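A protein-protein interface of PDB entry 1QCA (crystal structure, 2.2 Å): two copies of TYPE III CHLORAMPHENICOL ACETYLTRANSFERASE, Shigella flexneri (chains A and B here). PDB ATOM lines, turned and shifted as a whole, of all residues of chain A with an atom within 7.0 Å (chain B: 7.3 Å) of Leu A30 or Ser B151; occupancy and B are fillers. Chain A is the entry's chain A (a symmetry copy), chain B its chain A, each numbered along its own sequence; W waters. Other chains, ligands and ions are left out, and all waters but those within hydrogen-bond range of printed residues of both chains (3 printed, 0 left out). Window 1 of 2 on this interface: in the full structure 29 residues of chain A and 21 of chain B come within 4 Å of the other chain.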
ATOM      1  N   PHE A  28      -7.522 -21.400  17.629  1.00  0.00           N
ATOM      2  CA  PHE A  28      -8.410 -21.628  18.798  1.00  0.00           C
ATOM      3  C   PHE A  28      -9.412 -22.693  18.360  1.00  0.00           C
ATOM      4  O   PHE A  28      -9.693 -22.909  17.134  1.00  0.00           O
ATOM      5  CB  PHE A  28      -9.147 -20.309  19.140  1.00  0.00           C
ATOM      6  CG  PHE A  28     -10.055 -19.631  18.159  1.00  0.00           C
ATOM      7  CD1 PHE A  28      -9.573 -18.661  17.265  1.00  0.00           C
ATOM      8  CD2 PHE A  28     -11.403 -19.894  18.130  1.00  0.00           C
ATOM      9  CE1 PHE A  28     -10.385 -17.964  16.347  1.00  0.00           C
ATOM     10  CE2 PHE A  28     -12.268 -19.266  17.239  1.00  0.00           C
ATOM     11  CZ  PHE A  28     -11.761 -18.277  16.385  1.00  0.00           C
ATOM     12  N   SER A  29     -10.062 -23.290  19.341  1.00  0.00           N
ATOM     13  CA  SER A  29     -11.139 -24.226  19.097  1.00  0.00           C
ATOM     14  C   SER A  29     -12.294 -23.713  19.991  1.00  0.00           C
ATOM     15  O   SER A  29     -12.078 -22.953  21.013  1.00  0.00           O
ATOM     16  CB  SER A  29     -10.900 -25.704  19.376  1.00  0.00           C
ATOM     17  OG  SER A  29     -10.484 -25.784  20.748  1.00  0.00           O
ATOM     18  N   LEU A  30     -13.462 -24.150  19.611  1.00  0.00           N
ATOM     19  CA  LEU A  30     -14.720 -23.845  20.344  1.00  0.00           C
ATOM     20  C   LEU A  30     -15.692 -24.978  20.066  1.00  0.00           C
ATOM     21  O   LEU A  30     -15.733 -25.437  18.896  1.00  0.00           O
ATOM     22  CB  LEU A  30     -15.228 -22.482  20.018  1.00  0.00           C
ATOM     23  CG  LEU A  30     -16.199 -21.958  19.043  1.00  0.00           C
ATOM     24  CD1 LEU A  30     -17.632 -22.507  19.258  1.00  0.00           C
ATOM     25  CD2 LEU A  30     -16.343 -20.419  19.182  1.00  0.00           C
ATOM     26  N   THR A  31     -16.418 -25.435  21.021  1.00  0.00           N
ATOM     27  CA  THR A  31     -17.430 -26.445  20.915  1.00  0.00           C
ATOM     28  C   THR A  31     -18.770 -25.792  21.300  1.00  0.00           C
ATOM     29  O   THR A  31     -18.860 -25.132  22.385  1.00  0.00           O
ATOM     30  CB  THR A  31     -17.220 -27.690  21.830  1.00  0.00           C
ATOM     31  OG1 THR A  31     -15.824 -27.970  21.623  1.00  0.00           O
ATOM     32  CG2 THR A  31     -18.173 -28.802  21.437  1.00  0.00           C
ATOM     33  N   SER A  32     -19.726 -26.050  20.410  1.00  0.00           N
ATOM     34  CA  SER A  32     -21.047 -25.447  20.646  1.00  0.00           C
ATOM     35  C   SER A  32     -22.042 -26.558  20.364  1.00  0.00           C
ATOM     36  O   SER A  32     -21.575 -27.501  19.627  1.00  0.00           O
ATOM     37  CB  SER A  32     -21.121 -24.303  19.613  1.00  0.00           C
ATOM     38  OG  SER A  32     -22.342 -23.657  19.829  1.00  0.00           O
ATOM     39  N   ASP A 150     -18.490 -32.390  25.578  1.00  0.00           N
ATOM     40  CA  ASP A 150     -18.861 -30.978  25.716  1.00  0.00           C
ATOM     41  C   ASP A 150     -17.703 -30.151  25.113  1.00  0.00           C
ATOM     42  O   ASP A 150     -17.951 -28.962  24.913  1.00  0.00           O
ATOM     43  CB  ASP A 150     -19.138 -30.495  27.162  1.00  0.00           C
ATOM     44  CG  ASP A 150     -20.283 -31.357  27.702  1.00  0.00           C
ATOM     45  OD1 ASP A 150     -21.368 -31.049  27.214  1.00  0.00           O
ATOM     46  OD2 ASP A 150     -20.150 -32.323  28.466  1.00  0.00           O
ATOM     47  N   SER A 151     -16.576 -30.795  24.962  1.00  0.00           N
ATOM     48  CA  SER A 151     -15.449 -30.093  24.398  1.00  0.00           C
ATOM     49  C   SER A 151     -14.517 -31.064  23.703  1.00  0.00           C
ATOM     50  O   SER A 151     -14.405 -32.212  24.203  1.00  0.00           O
ATOM     51  CB  SER A 151     -14.636 -29.353  25.460  1.00  0.00           C
ATOM     52  OG  SER A 151     -13.784 -30.223  26.058  1.00  0.00           O
ATOM     53  N   PHE A 152     -13.794 -30.538  22.712  1.00  0.00           N
ATOM     54  CA  PHE A 152     -12.821 -31.301  21.993  1.00  0.00           C
ATOM     55  C   PHE A 152     -11.728 -30.314  21.563  1.00  0.00           C
ATOM     56  O   PHE A 152     -12.139 -29.305  20.996  1.00  0.00           O
ATOM     57  CB  PHE A 152     -13.458 -32.048  20.805  1.00  0.00           C
ATOM     58  CG  PHE A 152     -12.410 -32.883  20.126  1.00  0.00           C
ATOM     59  CD1 PHE A 152     -12.146 -34.177  20.580  1.00  0.00           C
ATOM     60  CD2 PHE A 152     -11.683 -32.386  19.054  1.00  0.00           C
ATOM     61  CE1 PHE A 152     -11.220 -35.027  19.980  1.00  0.00           C
ATOM     62  CE2 PHE A 152     -10.751 -33.194  18.387  1.00  0.00           C
ATOM     63  CZ  PHE A 152     -10.515 -34.494  18.912  1.00  0.00           C
ATOM     64  N   ASN A 153     -10.464 -30.594  21.758  1.00  0.00           N
ATOM     65  CA  ASN A 153      -9.414 -29.676  21.245  1.00  0.00           C
ATOM     66  C   ASN A 153      -8.252 -30.491  20.700  1.00  0.00           C
ATOM     67  O   ASN A 153      -7.880 -31.434  21.445  1.00  0.00           O
ATOM     68  CB  ASN A 153      -8.999 -28.674  22.322  1.00  0.00           C
ATOM     69  CG  ASN A 153      -7.834 -27.762  21.901  1.00  0.00           C
ATOM     70  OD1 ASN A 153      -6.636 -27.976  22.274  1.00  0.00           O
ATOM     71  ND2 ASN A 153      -8.130 -26.732  21.093  1.00  0.00           N
ATOM     72  N   LEU A 183     -20.450 -29.963  18.389  1.00  0.00           N
ATOM     73  CA  LEU A 183     -19.613 -29.726  17.231  1.00  0.00           C
ATOM     74  C   LEU A 183     -18.512 -28.753  17.623  1.00  0.00           C
ATOM     75  O   LEU A 183     -18.730 -27.631  18.130  1.00  0.00           O
ATOM     76  CB  LEU A 183     -20.507 -29.130  16.177  1.00  0.00           C
ATOM     77  CG  LEU A 183     -19.825 -28.770  14.883  1.00  0.00           C
ATOM     78  CD1 LEU A 183     -20.361 -29.722  13.828  1.00  0.00           C
ATOM     79  CD2 LEU A 183     -20.216 -27.315  14.666  1.00  0.00           C
ATOM     80  N   SER A 184     -17.278 -29.267  17.417  1.00  0.00           N
ATOM     81  CA  SER A 184     -16.038 -28.535  17.678  1.00  0.00           C
ATOM     82  C   SER A 184     -15.499 -28.007  16.354  1.00  0.00           C
ATOM     83  O   SER A 184     -15.479 -28.674  15.351  1.00  0.00           O
ATOM     84  CB  SER A 184     -15.085 -29.441  18.442  1.00  0.00           C
ATOM     85  OG  SER A 184     -13.976 -28.622  18.806  1.00  0.00           O
ATOM     86  N   VAL A 185     -15.028 -26.775  16.446  1.00  0.00           N
ATOM     87  CA  VAL A 185     -14.470 -26.091  15.289  1.00  0.00           C
ATOM     88  C   VAL A 185     -13.093 -25.564  15.705  1.00  0.00           C
ATOM     89  O   VAL A 185     -13.014 -24.826  16.684  1.00  0.00           O
ATOM     90  CB  VAL A 185     -15.402 -24.920  14.807  1.00  0.00           C
ATOM     91  CG1 VAL A 185     -14.761 -24.221  13.627  1.00  0.00           C
ATOM     92  CG2 VAL A 185     -16.798 -25.384  14.488  1.00  0.00           C
ATOM     93  N   GLN A 186     -12.080 -25.871  14.921  1.00  0.00           N
ATOM     94  CA  GLN A 186     -10.700 -25.411  15.218  1.00  0.00           C
ATOM     95  C   GLN A 186     -10.183 -24.672  13.997  1.00  0.00           C
ATOM     96  O   GLN A 186     -10.259 -25.196  12.839  1.00  0.00           O
ATOM     97  CB  GLN A 186      -9.919 -26.700  15.519  1.00  0.00           C
ATOM     98  CG  GLN A 186      -8.530 -26.292  16.015  1.00  0.00           C
ATOM     99  CD  GLN A 186      -7.977 -27.187  17.099  1.00  0.00           C
ATOM    100  OE1 GLN A 186      -8.670 -27.933  17.749  1.00  0.00           O
ATOM    101  NE2 GLN A 186      -6.667 -27.181  17.308  1.00  0.00           N
ATOM    102  N   VAL A 187      -9.750 -23.459  14.200  1.00  0.00           N
ATOM    103  CA  VAL A 187      -9.240 -22.650  13.056  1.00  0.00           C
ATOM    104  C   VAL A 187      -7.965 -21.901  13.500  1.00  0.00           C
ATOM    105  O   VAL A 187      -7.645 -21.783  14.727  1.00  0.00           O
ATOM    106  CB  VAL A 187     -10.335 -21.620  12.685  1.00  0.00           C
ATOM    107  CG1 VAL A 187     -11.593 -22.237  12.151  1.00  0.00           C
ATOM    108  CG2 VAL A 187     -10.717 -20.767  13.901  1.00  0.00           C
ATOM    109  N   GLY A 194     -13.333 -14.753  16.046  1.00  0.00           N
ATOM    110  CA  GLY A 194     -14.444 -15.389  16.744  1.00  0.00           C
ATOM    111  C   GLY A 194     -15.737 -15.060  15.990  1.00  0.00           C
ATOM    112  O   GLY A 194     -16.559 -15.962  15.975  1.00  0.00           O
ATOM    113  N   VAL A 197     -16.191 -17.583  13.201  1.00  0.00           N
ATOM    114  CA  VAL A 197     -16.601 -18.907  13.623  1.00  0.00           C
ATOM    115  C   VAL A 197     -18.085 -18.905  14.026  1.00  0.00           C
ATOM    116  O   VAL A 197     -18.792 -19.881  13.666  1.00  0.00           O
ATOM    117  CB  VAL A 197     -15.635 -19.456  14.686  1.00  0.00           C
ATOM    118  CG1 VAL A 197     -16.242 -20.749  15.271  1.00  0.00           C
ATOM    119  CG2 VAL A 197     -14.268 -19.730  14.028  1.00  0.00           C
ATOM    120  N   ALA A 198     -18.507 -17.874  14.734  1.00  0.00           N
ATOM    121  CA  ALA A 198     -19.909 -17.785  15.189  1.00  0.00           C
ATOM    122  C   ALA A 198     -20.815 -17.712  13.947  1.00  0.00           C
ATOM    123  O   ALA A 198     -21.867 -18.382  13.961  1.00  0.00           O
ATOM    124  CB  ALA A 198     -20.119 -16.665  16.180  1.00  0.00           C
ATOM    125  N   ILE A 201     -21.202 -21.317  12.434  1.00  0.00           N
ATOM    126  CA  ILE A 201     -22.080 -22.099  13.318  1.00  0.00           C
ATOM    127  C   ILE A 201     -23.534 -21.622  13.148  1.00  0.00           C
ATOM    128  O   ILE A 201     -24.401 -22.460  12.938  1.00  0.00           O
ATOM    129  CB  ILE A 201     -21.596 -21.949  14.797  1.00  0.00           C
ATOM    130  CG1 ILE A 201     -20.257 -22.733  14.884  1.00  0.00           C
ATOM    131  CG2 ILE A 201     -22.718 -22.372  15.745  1.00  0.00           C
ATOM    132  CD1 ILE A 201     -19.489 -22.579  16.226  1.00  0.00           C
ATOM    133  N   SER B  29      -6.626 -24.284  29.996  1.00  0.00           N
ATOM    134  CA  SER B  29      -7.824 -23.478  29.896  1.00  0.00           C
ATOM    135  C   SER B  29      -8.922 -24.351  30.552  1.00  0.00           C
ATOM    136  O   SER B  29      -8.796 -25.633  30.662  1.00  0.00           O
ATOM    137  CB  SER B  29      -8.290 -23.029  28.517  1.00  0.00           C
ATOM    138  OG  SER B  29      -8.440 -24.228  27.742  1.00  0.00           O
ATOM    139  N   LEU B  30      -9.957 -23.661  30.936  1.00  0.00           N
ATOM    140  CA  LEU B  30     -11.167 -24.281  31.540  1.00  0.00           C
ATOM    141  C   LEU B  30     -12.341 -23.364  31.244  1.00  0.00           C
ATOM    142  O   LEU B  30     -12.149 -22.124  31.335  1.00  0.00           O
ATOM    143  CB  LEU B  30     -10.961 -24.598  32.981  1.00  0.00           C
ATOM    144  CG  LEU B  30     -11.250 -23.887  34.237  1.00  0.00           C
ATOM    145  CD1 LEU B  30     -12.761 -23.621  34.451  1.00  0.00           C
ATOM    146  CD2 LEU B  30     -10.825 -24.739  35.463  1.00  0.00           C
ATOM    147  N   THR B  31     -13.469 -23.871  30.902  1.00  0.00           N
ATOM    148  CA  THR B  31     -14.689 -23.157  30.660  1.00  0.00           C
ATOM    149  C   THR B  31     -15.713 -23.636  31.704  1.00  0.00           C
ATOM    150  O   THR B  31     -15.910 -24.884  31.868  1.00  0.00           O
ATOM    151  CB  THR B  31     -15.308 -23.367  29.245  1.00  0.00           C
ATOM    152  OG1 THR B  31     -14.152 -23.232  28.399  1.00  0.00           O
ATOM    153  CG2 THR B  31     -16.417 -22.363  28.999  1.00  0.00           C
ATOM    154  N   SER B  32     -16.322 -22.619  32.311  1.00  0.00           N
ATOM    155  CA  SER B  32     -17.299 -22.947  33.360  1.00  0.00           C
ATOM    156  C   SER B  32     -18.482 -22.034  33.096  1.00  0.00           C
ATOM    157  O   SER B  32     -18.194 -20.998  32.394  1.00  0.00           O
ATOM    158  CB  SER B  32     -16.561 -22.603  34.672  1.00  0.00           C
ATOM    159  OG  SER B  32     -17.429 -22.948  35.712  1.00  0.00           O
ATOM    160  N   LYS B  33     -19.675 -22.347  33.583  1.00  0.00           N
ATOM    161  CA  LYS B  33     -20.761 -21.390  33.373  1.00  0.00           C
ATOM    162  C   LYS B  33     -21.002 -20.603  34.641  1.00  0.00           C
ATOM    163  O   LYS B  33     -21.034 -21.192  35.754  1.00  0.00           O
ATOM    164  CB  LYS B  33     -22.049 -22.015  32.908  1.00  0.00           C
ATOM    165  CG  LYS B  33     -21.902 -22.568  31.480  1.00  0.00           C
ATOM    166  CD  LYS B  33     -23.002 -23.584  31.167  1.00  0.00           C
ATOM    167  CE  LYS B  33     -23.113 -23.621  29.644  1.00  0.00           C
ATOM    168  NZ  LYS B  33     -22.049 -24.492  29.118  1.00  0.00           N
ATOM    169  N   LEU B 144     -17.408 -13.083  22.596  1.00  0.00           N
ATOM    170  CA  LEU B 144     -17.998 -13.729  21.446  1.00  0.00           C
ATOM    171  C   LEU B 144     -19.503 -13.655  21.694  1.00  0.00           C
ATOM    172  O   LEU B 144     -20.138 -14.685  22.017  1.00  0.00           O
ATOM    173  CB  LEU B 144     -17.473 -15.187  21.345  1.00  0.00           C
ATOM    174  CG  LEU B 144     -16.240 -15.414  20.497  1.00  0.00           C
ATOM    175  CD1 LEU B 144     -15.024 -14.992  21.343  1.00  0.00           C
ATOM    176  CD2 LEU B 144     -15.961 -16.816  20.122  1.00  0.00           C
ATOM    177  N   VAL B 147     -22.529 -16.179  19.720  1.00  0.00           N
ATOM    178  CA  VAL B 147     -22.755 -17.619  19.815  1.00  0.00           C
ATOM    179  C   VAL B 147     -22.454 -18.133  21.193  1.00  0.00           C
ATOM    180  O   VAL B 147     -21.495 -17.684  21.821  1.00  0.00           O
ATOM    181  CB  VAL B 147     -21.832 -18.456  18.825  1.00  0.00           C
ATOM    182  CG1 VAL B 147     -20.355 -18.533  19.196  1.00  0.00           C
ATOM    183  CG2 VAL B 147     -22.225 -19.905  18.653  1.00  0.00           C
ATOM    184  N   ASN B 148     -23.168 -19.138  21.591  1.00  0.00           N
ATOM    185  CA  ASN B 148     -22.964 -19.810  22.875  1.00  0.00           C
ATOM    186  C   ASN B 148     -21.889 -20.884  22.635  1.00  0.00           C
ATOM    187  O   ASN B 148     -21.836 -21.419  21.522  1.00  0.00           O
ATOM    188  CB  ASN B 148     -24.266 -20.456  23.333  1.00  0.00           C
ATOM    189  CG  ASN B 148     -24.192 -20.961  24.775  1.00  0.00           C
ATOM    190  OD1 ASN B 148     -24.112 -22.209  24.917  1.00  0.00           O
ATOM    191  ND2 ASN B 148     -24.211 -20.147  25.835  1.00  0.00           N
ATOM    192  N   PHE B 149     -21.062 -21.202  23.601  1.00  0.00           N
ATOM    193  CA  PHE B 149     -20.030 -22.225  23.461  1.00  0.00           C
ATOM    194  C   PHE B 149     -19.971 -22.896  24.845  1.00  0.00           C
ATOM    195  O   PHE B 149     -20.279 -22.294  25.840  1.00  0.00           O
ATOM    196  CB  PHE B 149     -18.644 -21.806  22.989  1.00  0.00           C
ATOM    197  CG  PHE B 149     -17.852 -20.776  23.773  1.00  0.00           C
ATOM    198  CD1 PHE B 149     -17.462 -20.988  25.079  1.00  0.00           C
ATOM    199  CD2 PHE B 149     -17.409 -19.609  23.165  1.00  0.00           C
ATOM    200  CE1 PHE B 149     -16.722 -20.060  25.818  1.00  0.00           C
ATOM    201  CE2 PHE B 149     -16.654 -18.684  23.883  1.00  0.00           C
ATOM    202  CZ  PHE B 149     -16.329 -18.890  25.216  1.00  0.00           C
ATOM    203  N   ASP B 150     -19.512 -24.149  24.832  1.00  0.00           N
ATOM    204  CA  ASP B 150     -19.329 -24.910  26.074  1.00  0.00           C
ATOM    205  C   ASP B 150     -17.811 -24.941  26.359  1.00  0.00           C
ATOM    206  O   ASP B 150     -17.492 -25.317  27.488  1.00  0.00           O
ATOM    207  CB  ASP B 150     -19.879 -26.357  26.061  1.00  0.00           C
ATOM    208  CG  ASP B 150     -21.379 -26.256  25.765  1.00  0.00           C
ATOM    209  OD1 ASP B 150     -22.017 -25.846  26.731  1.00  0.00           O
ATOM    210  OD2 ASP B 150     -21.904 -26.463  24.662  1.00  0.00           O
ATOM    211  N   SER B 151     -17.046 -24.641  25.343  1.00  0.00           N
ATOM    212  CA  SER B 151     -15.615 -24.641  25.532  1.00  0.00           C
ATOM    213  C   SER B 151     -14.954 -23.687  24.558  1.00  0.00           C
ATOM    214  O   SER B 151     -15.477 -23.575  23.420  1.00  0.00           O
ATOM    215  CB  SER B 151     -15.002 -26.024  25.311  1.00  0.00           C
ATOM    216  OG  SER B 151     -14.817 -26.225  23.983  1.00  0.00           O
ATOM    217  N   PHE B 152     -13.790 -23.181  24.969  1.00  0.00           N
ATOM    218  CA  PHE B 152     -13.006 -22.313  24.146  1.00  0.00           C
ATOM    219  C   PHE B 152     -11.540 -22.563  24.525  1.00  0.00           C
ATOM    220  O   PHE B 152     -11.304 -22.513  25.730  1.00  0.00           O
ATOM    221  CB  PHE B 152     -13.429 -20.842  24.318  1.00  0.00           C
ATOM    222  CG  PHE B 152     -12.622 -19.982  23.386  1.00  0.00           C
ATOM    223  CD1 PHE B 152     -13.055 -19.776  22.074  1.00  0.00           C
ATOM    224  CD2 PHE B 152     -11.437 -19.392  23.802  1.00  0.00           C
ATOM    225  CE1 PHE B 152     -12.385 -18.963  21.163  1.00  0.00           C
ATOM    226  CE2 PHE B 152     -10.723 -18.542  22.945  1.00  0.00           C
ATOM    227  CZ  PHE B 152     -11.208 -18.392  21.617  1.00  0.00           C
ATOM    228  N   ASN B 153     -10.637 -22.758  23.599  1.00  0.00           N
ATOM    229  CA  ASN B 153      -9.206 -22.897  23.976  1.00  0.00           C
ATOM    230  C   ASN B 153      -8.340 -22.179  22.954  1.00  0.00           C
ATOM    231  O   ASN B 153      -8.645 -22.409  21.756  1.00  0.00           O
ATOM    232  CB  ASN B 153      -8.836 -24.369  24.156  1.00  0.00           C
ATOM    233  CG  ASN B 153      -7.341 -24.600  24.438  1.00  0.00           C
ATOM    234  OD1 ASN B 153      -6.529 -24.973  23.531  1.00  0.00           O
ATOM    235  ND2 ASN B 153      -6.915 -24.366  25.689  1.00  0.00           N
ATOM    236  N   ASN B 155      -4.758 -22.029  21.045  1.00  0.00           N
ATOM    237  CA  ASN B 155      -3.596 -22.884  20.754  1.00  0.00           C
ATOM    238  C   ASN B 155      -2.504 -21.917  20.331  1.00  0.00           C
ATOM    239  O   ASN B 155      -2.596 -21.339  19.243  1.00  0.00           O
ATOM    240  CB  ASN B 155      -4.061 -23.809  19.648  1.00  0.00           C
ATOM    241  CG  ASN B 155      -5.174 -24.726  20.161  1.00  0.00           C
ATOM    242  OD1 ASN B 155      -6.261 -24.745  19.572  1.00  0.00           O
ATOM    243  ND2 ASN B 155      -4.888 -25.496  21.216  1.00  0.00           N
ATOM    244  N   PRO B 182     -21.167 -18.721  29.689  1.00  0.00           N
ATOM    245  CA  PRO B 182     -19.942 -19.522  29.519  1.00  0.00           C
ATOM    246  C   PRO B 182     -18.757 -18.507  29.570  1.00  0.00           C
ATOM    247  O   PRO B 182     -18.741 -17.446  28.913  1.00  0.00           O
ATOM    248  CB  PRO B 182     -20.071 -20.137  28.137  1.00  0.00           C
ATOM    249  CG  PRO B 182     -21.573 -20.112  27.821  1.00  0.00           C
ATOM    250  CD  PRO B 182     -21.920 -18.677  28.425  1.00  0.00           C
ATOM    251  N   SER B 184     -14.441 -18.780  29.660  1.00  0.00           N
ATOM    252  CA  SER B 184     -13.190 -19.522  29.512  1.00  0.00           C
ATOM    253  C   SER B 184     -12.066 -18.705  30.140  1.00  0.00           C
ATOM    254  O   SER B 184     -11.961 -17.517  29.976  1.00  0.00           O
ATOM    255  CB  SER B 184     -12.991 -19.863  28.044  1.00  0.00           C
ATOM    256  OG  SER B 184     -11.852 -20.718  27.992  1.00  0.00           O
HETATM  257  O   HOH W   1      -6.178 -24.156  16.554  1.00  0.00           O
HETATM  258  O   HOH W   2     -21.081 -28.760  23.369  1.00  0.00           O
HETATM  259  O   HOH W   3     -12.609 -26.225  22.836  1.00  0.00           O
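Ser A29 touches Phe B152, but with the chains exchanged Phe A152 does not touch Ser B29 (9.2 Å). Leu A30 touches Ser B151, but with the chains exchanged Ser A151 does not touch Leu B30 (8.5 Å). Thr A31 touches Ser B151, but with the chains exchanged Ser A151 does not touch Thr B31 (6.8 Å). Ser B151 touches its own counterpart, Ser A151. Of the 21 pairs that touch across the chains among the printed residues, 3 have their exchanged pair printed and touching as well.
ND2 of Asn B153 is in hydrogen-bond range of OG of Ser B29 (2.6 Å). The side-chain hydroxyl of Thr B31 lies within hydrogen-bond range of the backbone NH of Phe B152. NZ of Lys B33 is in salt-bridge range of OD1 of Asp B150 (2.7 Å). The backbone carbonyl oxygen of Phe B152 is in hydrogen-bond range of the side-chain hydroxyl of Ser B184. The side-chain amide oxygen (OD1) of Asn B153 lies within hydrogen-bond range of the side-chain amide nitrogen (ND2) of Asn B155, at 2.9 Å. The backbone NH (N) of Val A185 is in hydrogen-bond range of the backbone carbonyl oxygen (O) of Leu A30.
Of the printed residues of chain B, Phe A28 touches Phe B152, Asn B153 and Asn B155. Of the printed residues of chain B, Asp A150 touches Asp B150 (3.4 Å). Phe A152 touches none of the printed residues of chain B. Printed residues of chain B within 4 Å of Gln A186: Asn B155. The nearest printed residue of chain A that does not touch Ser B151 is Asp A150 (4.2 Å).
O of Asn B148 sits at hydrogen-bond distance from OG of Ser A32, at 2.9 Å. The backbone NH (N) of Asp B150 lies within hydrogen-bond range of the backbone carbonyl oxygen (O) of Thr A31, at 2.7 Å. The side-chain hydroxyl (OG) of Ser B151 is in hydrogen-bond range of the side-chain hydroxyl (OG1) of Thr A31. O of Asn B153 lies within hydrogen-bond range of N of Ser A29. OD1 of Asn B153 lies close to OD1 of Asn A153, at 3.3 Å. The side-chain amide nitrogen (ND2) of Asn A153 is in hydrogen-bond range of the side-chain amide oxygen (OD1) of Asn B155 (3.1 Å). NE2 of Gln A186 sits at hydrogen-bond distance from OD1 of Asn B155 (3.4 Å).
Water W3 lies within hydrogen-bond range of OG of Ser B151 (2.5 Å) and OG of Ser A29 (3.0 Å). Water W2 bridges the side-chain carboxylate of Asp B150 (2.8 Å) and the backbone carbonyl oxygen of Asp A150 (3.5 Å). Water W1 lies within hydrogen-bond range of OD1 of Asn B155, NE2 of Gln A186, N of Phe A28 and O of Val A187.
Of the 18 printed residues of chain A, 12 touch a printed residue of chain B. Along chain A the printed residues that touch a printed residue of chain B span positions 28 to 201. Hydrophobic or aromatic side chains of chain B within 4 Å of the printed part of chain A: Leu B144, Val B147, Phe B149 and Phe B152. Among the printed residues, no Asp or Glu carboxylate lies within 4 Å of a Lys or Arg side-chain nitrogen of the other chain.
Among the printed residues, pairs that only touch across the chains: Phe A28 with Phe B152, Phe A28 with Asn B153, Phe A28 with Asn B155, Ser A29 with Phe B152, Leu A30 with Leu B144, Leu A30 with Phe B149, Leu A30 with Ser B151, Thr A31 with Phe B149, Ser A32 with Val B147, Asp A150 with Asp B150, Ser A151 with Ser B151, Gly A194 with Leu B144, Ala A198 with Val B147 and Ile A201 with Val B147.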
